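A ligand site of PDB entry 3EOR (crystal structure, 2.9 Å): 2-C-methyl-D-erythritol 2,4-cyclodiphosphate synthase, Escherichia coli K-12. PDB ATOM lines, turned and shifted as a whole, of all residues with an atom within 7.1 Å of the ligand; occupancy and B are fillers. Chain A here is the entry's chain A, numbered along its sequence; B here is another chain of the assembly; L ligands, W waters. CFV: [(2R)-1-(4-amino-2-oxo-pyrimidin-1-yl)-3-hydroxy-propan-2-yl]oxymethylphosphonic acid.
NAF of the ligand lies within hydrogen-bond range of O of Pro 109 (2.8 Å).
The backbone NH (N) of Leu 112 sits at hydrogen-bond distance from an oxygen (OAI) of the ligand (2.8 Å).
N of Met 111 is in hydrogen-bond range of NAG of the ligand (2.8 Å).
NAF of the ligand lies within hydrogen-bond range of O of Ala 106, 3.1 Å away.
The backbone carbonyl oxygen (O) of Thr 138 sits at hydrogen-bond distance from the backbone NH (N) of Ala 106, at 3.1 Å.
OG1 of Thr 139 lies within hydrogen-bond range of N of Glu 141 (3.2 Å).
N of Gly 64 of chain B lies within hydrogen-bond range of OD2 of Asp 62 of chain B (3.0 Å).
N of Thr 138 is in hydrogen-bond range of O of Ile 104, at 2.7 Å.
Water W2 lies within hydrogen-bond range of OAP of the ligand, N of Thr 139 and OG1 of Thr 138.
CG of Lys 110 touches OAI of the ligand (3.4 Å).
Ala 137 touches the ligand.
Thr 138 touches the ligand (N to CAC, 3.9 Å).
CG2 of Thr 139 touches CAD of the ligand (3.7 Å).
Gly 64 of chain B touches the ligand.
Hydrophobic or aromatic side chains that line the ligand: Met 111, Leu 112 and Ala 137.
Of the 25 residues printed, 9 come within 4 Å of the ligand.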
ATOM      1  N   ILE A 104      -6.224 -14.236   1.817  1.00  0.00           N
ATOM      2  CA  ILE A 104      -5.495 -13.460   2.796  1.00  0.00           C
ATOM      3  C   ILE A 104      -6.333 -13.438   4.103  1.00  0.00           C
ATOM      4  O   ILE A 104      -7.536 -13.262   4.073  1.00  0.00           O
ATOM      5  CB  ILE A 104      -5.268 -12.032   2.311  1.00  0.00           C
ATOM      6  CG1 ILE A 104      -4.639 -12.039   0.932  1.00  0.00           C
ATOM      7  CG2 ILE A 104      -4.437 -11.204   3.341  1.00  0.00           C
ATOM      8  CD1 ILE A 104      -4.773 -10.688   0.203  1.00  0.00           C
ATOM      9  N   ILE A 105      -5.671 -13.636   5.234  1.00  0.00           N
ATOM     10  CA  ILE A 105      -6.323 -13.703   6.535  1.00  0.00           C
ATOM     11  C   ILE A 105      -5.745 -12.562   7.419  1.00  0.00           C
ATOM     12  O   ILE A 105      -4.619 -12.648   7.905  1.00  0.00           O
ATOM     13  CB  ILE A 105      -6.113 -15.082   7.221  1.00  0.00           C
ATOM     14  CG1 ILE A 105      -6.496 -16.223   6.265  1.00  0.00           C
ATOM     15  CG2 ILE A 105      -6.841 -15.110   8.625  1.00  0.00           C
ATOM     16  CD1 ILE A 105      -6.093 -17.524   6.723  1.00  0.00           C
ATOM     17  N   ALA A 106      -6.498 -11.476   7.616  1.00  0.00           N
ATOM     18  CA  ALA A 106      -5.961 -10.313   8.273  1.00  0.00           C
ATOM     19  C   ALA A 106      -7.140  -9.526   8.835  1.00  0.00           C
ATOM     20  O   ALA A 106      -8.223  -9.468   8.221  1.00  0.00           O
ATOM     21  CB  ALA A 106      -5.225  -9.481   7.284  1.00  0.00           C
ATOM     22  N   GLN A 107      -6.950  -8.936  10.011  1.00  0.00           N
ATOM     23  CA  GLN A 107      -7.970  -8.078  10.620  1.00  0.00           C
ATOM     24  C   GLN A 107      -7.962  -6.692   9.932  1.00  0.00           C
ATOM     25  O   GLN A 107      -9.000  -6.149   9.651  1.00  0.00           O
ATOM     26  CB  GLN A 107      -7.705  -7.934  12.129  1.00  0.00           C
ATOM     27  CG  GLN A 107      -8.845  -7.382  12.909  1.00  0.00           C
ATOM     28  CD  GLN A 107     -10.046  -8.363  12.987  1.00  0.00           C
ATOM     29  OE1 GLN A 107      -9.903  -9.593  13.063  1.00  0.00           O
ATOM     30  NE2 GLN A 107     -11.256  -7.790  12.967  1.00  0.00           N
ATOM     31  N   ALA A 108      -6.763  -6.131   9.702  1.00  0.00           N
ATOM     32  CA  ALA A 108      -6.584  -5.058   8.758  1.00  0.00           C
ATOM     33  C   ALA A 108      -5.164  -5.121   8.173  1.00  0.00           C
ATOM     34  O   ALA A 108      -4.304  -5.853   8.690  1.00  0.00           O
ATOM     35  CB  ALA A 108      -6.810  -3.798   9.431  1.00  0.00           C
ATOM     36  N   PRO A 109      -4.898  -4.330   7.130  1.00  0.00           N
ATOM     37  CA  PRO A 109      -5.896  -3.378   6.645  1.00  0.00           C
ATOM     38  C   PRO A 109      -6.915  -3.999   5.717  1.00  0.00           C
ATOM     39  O   PRO A 109      -6.868  -5.203   5.458  1.00  0.00           O
ATOM     40  CB  PRO A 109      -5.054  -2.387   5.845  1.00  0.00           C
ATOM     41  CG  PRO A 109      -3.809  -3.142   5.456  1.00  0.00           C
ATOM     42  CD  PRO A 109      -3.560  -4.152   6.508  1.00  0.00           C
ATOM     43  N   LYS A 110      -7.794  -3.170   5.160  1.00  0.00           N
ATOM     44  CA  LYS A 110      -8.795  -3.647   4.204  1.00  0.00           C
ATOM     45  C   LYS A 110      -8.126  -3.991   2.878  1.00  0.00           C
ATOM     46  O   LYS A 110      -7.536  -3.121   2.269  1.00  0.00           O
ATOM     47  CB  LYS A 110      -9.898  -2.592   4.013  1.00  0.00           C
ATOM     48  CG  LYS A 110     -11.101  -3.124   3.250  1.00  0.00           C
ATOM     49  CD  LYS A 110     -12.360  -2.439   3.678  1.00  0.00           C
ATOM     50  CE  LYS A 110     -12.634  -1.145   2.841  1.00  0.00           C
ATOM     51  NZ  LYS A 110     -13.372  -1.514   1.571  1.00  0.00           N
ATOM     52  N   MET A 111      -8.231  -5.227   2.426  1.00  0.00           N
ATOM     53  CA  MET A 111      -7.575  -5.670   1.228  1.00  0.00           C
ATOM     54  C   MET A 111      -8.426  -5.438  -0.005  1.00  0.00           C
ATOM     55  O   MET A 111      -7.930  -5.354  -1.132  1.00  0.00           O
ATOM     56  CB  MET A 111      -7.216  -7.146   1.324  1.00  0.00           C
ATOM     57  CG  MET A 111      -6.427  -7.562   2.552  1.00  0.00           C
ATOM     58  SD  MET A 111      -4.743  -6.921   2.535  1.00  0.00           S
ATOM     59  CE  MET A 111      -4.196  -7.063   4.262  1.00  0.00           C
ATOM     60  N   LEU A 112      -9.718  -5.324   0.195  1.00  0.00           N
ATOM     61  CA  LEU A 112     -10.669  -5.517  -0.881  1.00  0.00           C
ATOM     62  C   LEU A 112     -10.421  -4.597  -2.067  1.00  0.00           C
ATOM     63  O   LEU A 112     -10.440  -5.036  -3.226  1.00  0.00           O
ATOM     64  CB  LEU A 112     -12.107  -5.315  -0.380  1.00  0.00           C
ATOM     65  CG  LEU A 112     -13.241  -5.514  -1.382  1.00  0.00           C
ATOM     66  CD1 LEU A 112     -13.145  -6.928  -1.995  1.00  0.00           C
ATOM     67  CD2 LEU A 112     -14.571  -5.253  -0.764  1.00  0.00           C
ATOM     68  N   PRO A 113     -10.238  -3.301  -1.812  1.00  0.00           N
ATOM     69  CA  PRO A 113     -10.073  -2.326  -2.908  1.00  0.00           C
ATOM     70  C   PRO A 113      -8.793  -2.576  -3.728  1.00  0.00           C
ATOM     71  O   PRO A 113      -8.694  -2.115  -4.862  1.00  0.00           O
ATOM     72  CB  PRO A 113      -9.941  -1.006  -2.160  1.00  0.00           C
ATOM     73  CG  PRO A 113      -9.390  -1.394  -0.840  1.00  0.00           C
ATOM     74  CD  PRO A 113     -10.028  -2.682  -0.498  1.00  0.00           C
ATOM     75  N   ILE A 115      -7.648  -5.417  -4.627  1.00  0.00           N
ATOM     76  CA  ILE A 115      -7.657  -6.819  -4.943  1.00  0.00           C
ATOM     77  C   ILE A 115      -7.649  -7.038  -6.458  1.00  0.00           C
ATOM     78  O   ILE A 115      -7.188  -8.083  -6.923  1.00  0.00           O
ATOM     79  CB  ILE A 115      -8.853  -7.565  -4.320  1.00  0.00           C
ATOM     80  CG1 ILE A 115      -8.435  -8.183  -2.995  1.00  0.00           C
ATOM     81  CG2 ILE A 115      -9.330  -8.686  -5.266  1.00  0.00           C
ATOM     82  CD1 ILE A 115      -9.464  -9.096  -2.341  1.00  0.00           C
ATOM     83  N   LYS A 136      -8.956 -13.461  -2.317  1.00  0.00           N
ATOM     84  CA  LYS A 136      -9.866 -12.908  -1.322  1.00  0.00           C
ATOM     85  C   LYS A 136      -9.187 -12.685  -0.023  1.00  0.00           C
ATOM     86  O   LYS A 136      -8.143 -13.235   0.222  1.00  0.00           O
ATOM     87  CB  LYS A 136     -11.087 -13.768  -1.123  1.00  0.00           C
ATOM     88  CG  LYS A 136     -10.880 -15.101  -0.489  1.00  0.00           C
ATOM     89  CD  LYS A 136     -11.693 -16.096  -1.193  1.00  0.00           C
ATOM     90  CE  LYS A 136     -11.187 -17.396  -0.929  1.00  0.00           C
ATOM     91  NZ  LYS A 136     -10.423 -18.044  -1.994  1.00  0.00           N
ATOM     92  N   ALA A 137      -9.776 -11.849   0.820  1.00  0.00           N
ATOM     93  CA  ALA A 137      -9.295 -11.677   2.177  1.00  0.00           C
ATOM     94  C   ALA A 137     -10.432 -11.891   3.148  1.00  0.00           C
ATOM     95  O   ALA A 137     -11.567 -11.609   2.832  1.00  0.00           O
ATOM     96  CB  ALA A 137      -8.694 -10.300   2.368  1.00  0.00           C
ATOM     97  N   THR A 138     -10.122 -12.382   4.338  1.00  0.00           N
ATOM     98  CA  THR A 138     -11.125 -12.707   5.314  1.00  0.00           C
ATOM     99  C   THR A 138     -10.606 -12.360   6.715  1.00  0.00           C
ATOM    100  O   THR A 138      -9.398 -12.316   6.878  1.00  0.00           O
ATOM    101  CB  THR A 138     -11.613 -14.192   5.212  1.00  0.00           C
ATOM    102  OG1 THR A 138     -12.673 -14.289   6.153  1.00  0.00           O
ATOM    103  CG2 THR A 138     -10.584 -15.179   5.683  1.00  0.00           C
ATOM    104  N   THR A 139     -11.486 -12.046   7.703  1.00  0.00           N
ATOM    105  CA  THR A 139     -10.946 -11.803   9.071  1.00  0.00           C
ATOM    106  C   THR A 139     -11.170 -13.045   9.899  1.00  0.00           C
ATOM    107  O   THR A 139     -11.965 -13.863   9.497  1.00  0.00           O
ATOM    108  CB  THR A 139     -11.550 -10.643   9.863  1.00  0.00           C
ATOM    109  OG1 THR A 139     -12.869 -10.995  10.240  1.00  0.00           O
ATOM    110  CG2 THR A 139     -11.606  -9.417   9.063  1.00  0.00           C
ATOM    111  N   THR A 140     -10.495 -13.151  11.045  1.00  0.00           N
ATOM    112  CA  THR A 140     -10.811 -14.162  12.014  1.00  0.00           C
ATOM    113  C   THR A 140     -11.518 -13.568  13.210  1.00  0.00           C
ATOM    114  O   THR A 140     -11.394 -14.059  14.344  1.00  0.00           O
ATOM    115  CB  THR A 140      -9.578 -14.886  12.486  1.00  0.00           C
ATOM    116  OG1 THR A 140      -8.690 -13.944  13.107  1.00  0.00           O
ATOM    117  CG2 THR A 140      -8.880 -15.571  11.312  1.00  0.00           C
ATOM    118  N   GLU A 141     -12.258 -12.476  12.969  1.00  0.00           N
ATOM    119  CA  GLU A 141     -13.262 -11.990  13.912  1.00  0.00           C
ATOM    120  C   GLU A 141     -12.650 -11.734  15.264  1.00  0.00           C
ATOM    121  O   GLU A 141     -13.265 -12.003  16.305  1.00  0.00           O
ATOM    122  CB  GLU A 141     -14.409 -12.998  14.044  1.00  0.00           C
ATOM    123  CG  GLU A 141     -15.140 -13.263  12.746  1.00  0.00           C
ATOM    124  CD  GLU A 141     -16.065 -12.171  12.341  1.00  0.00           C
ATOM    125  OE1 GLU A 141     -16.051 -11.128  13.006  1.00  0.00           O
ATOM    126  OE2 GLU A 141     -16.818 -12.366  11.352  1.00  0.00           O
ATOM    127  N   ILE A 152      -0.289 -11.423  10.011  1.00  0.00           N
ATOM    128  CA  ILE A 152      -1.057 -11.576   8.802  1.00  0.00           C
ATOM    129  C   ILE A 152      -0.759 -12.914   8.114  1.00  0.00           C
ATOM    130  O   ILE A 152       0.386 -13.227   7.800  1.00  0.00           O
ATOM    131  CB  ILE A 152      -0.728 -10.422   7.876  1.00  0.00           C
ATOM    132  CG1 ILE A 152      -1.811 -10.159   6.880  1.00  0.00           C
ATOM    133  CG2 ILE A 152       0.590 -10.691   7.060  1.00  0.00           C
ATOM    134  CD1 ILE A 152      -1.586  -8.765   6.296  1.00  0.00           C
ATOM    135  N   HIS B  40     -23.380 -11.466  11.827  1.00  0.00           N
ATOM    136  CA  HIS B  40     -24.452 -10.679  11.222  1.00  0.00           C
ATOM    137  C   HIS B  40     -25.406 -11.528  10.416  1.00  0.00           C
ATOM    138  O   HIS B  40     -26.148 -10.993   9.652  1.00  0.00           O
ATOM    139  CB  HIS B  40     -23.866  -9.522  10.385  1.00  0.00           C
ATOM    140  CG  HIS B  40     -23.376  -8.375  11.228  1.00  0.00           C
ATOM    141  ND1 HIS B  40     -24.250  -7.533  11.900  1.00  0.00           N
ATOM    142  CD2 HIS B  40     -22.128  -7.935  11.516  1.00  0.00           C
ATOM    143  CE1 HIS B  40     -23.554  -6.619  12.561  1.00  0.00           C
ATOM    144  NE2 HIS B  40     -22.267  -6.840  12.345  1.00  0.00           N
ATOM    145  N   ASP B  62     -15.584 -13.711  -3.661  1.00  0.00           N
ATOM    146  CA  ASP B  62     -16.027 -14.308  -2.373  1.00  0.00           C
ATOM    147  C   ASP B  62     -17.353 -13.719  -1.925  1.00  0.00           C
ATOM    148  O   ASP B  62     -17.769 -12.711  -2.469  1.00  0.00           O
ATOM    149  CB  ASP B  62     -14.990 -14.087  -1.302  1.00  0.00           C
ATOM    150  CG  ASP B  62     -14.755 -12.620  -1.016  1.00  0.00           C
ATOM    151  OD1 ASP B  62     -14.188 -11.913  -1.874  1.00  0.00           O
ATOM    152  OD2 ASP B  62     -15.137 -12.153   0.081  1.00  0.00           O
ATOM    153  N   ILE B  63     -17.988 -14.352  -0.937  1.00  0.00           N
ATOM    154  CA  ILE B  63     -19.179 -13.799  -0.309  1.00  0.00           C
ATOM    155  C   ILE B  63     -19.080 -12.283  -0.100  1.00  0.00           C
ATOM    156  O   ILE B  63     -19.897 -11.545  -0.632  1.00  0.00           O
ATOM    157  CB  ILE B  63     -19.409 -14.390   1.048  1.00  0.00           C
ATOM    158  CG1 ILE B  63     -19.392 -15.891   0.982  1.00  0.00           C
ATOM    159  CG2 ILE B  63     -20.793 -13.964   1.595  1.00  0.00           C
ATOM    160  CD1 ILE B  63     -19.462 -16.484   2.412  1.00  0.00           C
ATOM    161  N   GLY B  64     -18.076 -11.845   0.656  1.00  0.00           N
ATOM    162  CA  GLY B  64     -17.960 -10.463   1.087  1.00  0.00           C
ATOM    163  C   GLY B  64     -18.071  -9.459  -0.040  1.00  0.00           C
ATOM    164  O   GLY B  64     -18.744  -8.430   0.081  1.00  0.00           O
ATOM    165  N   LYS B  65     -17.409  -9.752  -1.158  1.00  0.00           N
ATOM    166  CA  LYS B  65     -17.643  -9.025  -2.406  1.00  0.00           C
ATOM    167  C   LYS B  65     -19.101  -9.191  -2.809  1.00  0.00           C
ATOM    168  O   LYS B  65     -19.859  -8.217  -2.766  1.00  0.00           O
ATOM    169  CB  LYS B  65     -16.715  -9.516  -3.526  1.00  0.00           C
ATOM    170  CG  LYS B  65     -16.726  -8.713  -4.796  1.00  0.00           C
ATOM    171  CD  LYS B  65     -15.305  -8.620  -5.309  1.00  0.00           C
ATOM    172  CE  LYS B  65     -15.289  -8.409  -6.792  1.00  0.00           C
ATOM    173  NZ  LYS B  65     -15.769  -9.624  -7.492  1.00  0.00           N
ATOM    174  N   PHE B  67     -21.788 -10.231  -1.574  1.00  0.00           N
ATOM    175  CA  PHE B  67     -22.858  -9.879  -0.645  1.00  0.00           C
ATOM    176  C   PHE B  67     -22.377  -9.026   0.538  1.00  0.00           C
ATOM    177  O   PHE B  67     -22.090  -9.531   1.629  1.00  0.00           O
ATOM    178  CB  PHE B  67     -23.527 -11.169  -0.120  1.00  0.00           C
ATOM    179  CG  PHE B  67     -23.705 -12.233  -1.165  1.00  0.00           C
ATOM    180  CD1 PHE B  67     -24.443 -11.985  -2.308  1.00  0.00           C
ATOM    181  CD2 PHE B  67     -23.138 -13.506  -1.011  1.00  0.00           C
ATOM    182  CE1 PHE B  67     -24.607 -12.960  -3.274  1.00  0.00           C
ATOM    183  CE2 PHE B  67     -23.298 -14.492  -1.985  1.00  0.00           C
ATOM    184  CZ  PHE B  67     -24.031 -14.202  -3.121  1.00  0.00           C
ATOM    185  N   PRO B  68     -22.280  -7.723   0.306  1.00  0.00           N
ATOM    186  CA  PRO B  68     -21.834  -6.775   1.339  1.00  0.00           C
ATOM    187  C   PRO B  68     -22.736  -6.829   2.569  1.00  0.00           C
ATOM    188  O   PRO B  68     -23.944  -6.645   2.452  1.00  0.00           O
ATOM    189  CB  PRO B  68     -21.958  -5.414   0.649  1.00  0.00           C
ATOM    190  CG  PRO B  68     -21.778  -5.721  -0.795  1.00  0.00           C
ATOM    191  CD  PRO B  68     -22.401  -7.068  -1.021  1.00  0.00           C
HETATM  192  OAN CFV L   1     -15.465  -6.846   7.794  1.00  0.00           O
HETATM  193  PAM CFV L   1     -15.870  -7.763   6.735  1.00  0.00           P
HETATM  194  OAO CFV L   1     -17.307  -7.945   6.578  1.00  0.00           O
HETATM  195  OAP CFV L   1     -15.101  -9.006   6.657  1.00  0.00           O
HETATM  196  CAL CFV L   1     -15.423  -6.838   5.277  1.00  0.00           C
HETATM  197  OAK CFV L   1     -14.059  -6.981   4.888  1.00  0.00           O
HETATM  198  CAJ CFV L   1     -14.085  -8.009   3.957  1.00  0.00           C
HETATM  199  CAQ CFV L   1     -15.015  -7.448   3.017  1.00  0.00           C
HETATM  200  OAR CFV L   1     -14.885  -8.233   1.868  1.00  0.00           O
HETATM  201  CAA CFV L   1     -12.916  -8.177   3.061  1.00  0.00           C
HETATM  202  NAB CFV L   1     -11.717  -8.042   3.833  1.00  0.00           N
HETATM  203  CAC CFV L   1     -11.501  -8.796   4.930  1.00  0.00           C
HETATM  204  CAD CFV L   1     -10.350  -8.610   5.630  1.00  0.00           C
HETATM  205  CAE CFV L   1      -9.472  -7.679   5.188  1.00  0.00           C
HETATM  206  NAF CFV L   1      -8.374  -7.480   5.839  1.00  0.00           N
HETATM  207  NAG CFV L   1      -9.716  -6.961   4.118  1.00  0.00           N
HETATM  208  CAH CFV L   1     -10.821  -7.143   3.454  1.00  0.00           C
HETATM  209  OAI CFV L   1     -11.096  -6.442   2.370  1.00  0.00           O
HETATM  210  O   HOH W   1     -18.809  -8.961   9.152  1.00  0.00           O
HETATM  211  O   HOH W   2     -14.153 -11.315   6.220  1.00  0.00           O
HETATM  212  O   HOH W   3     -12.881  -5.102   6.633  1.00  0.00           O
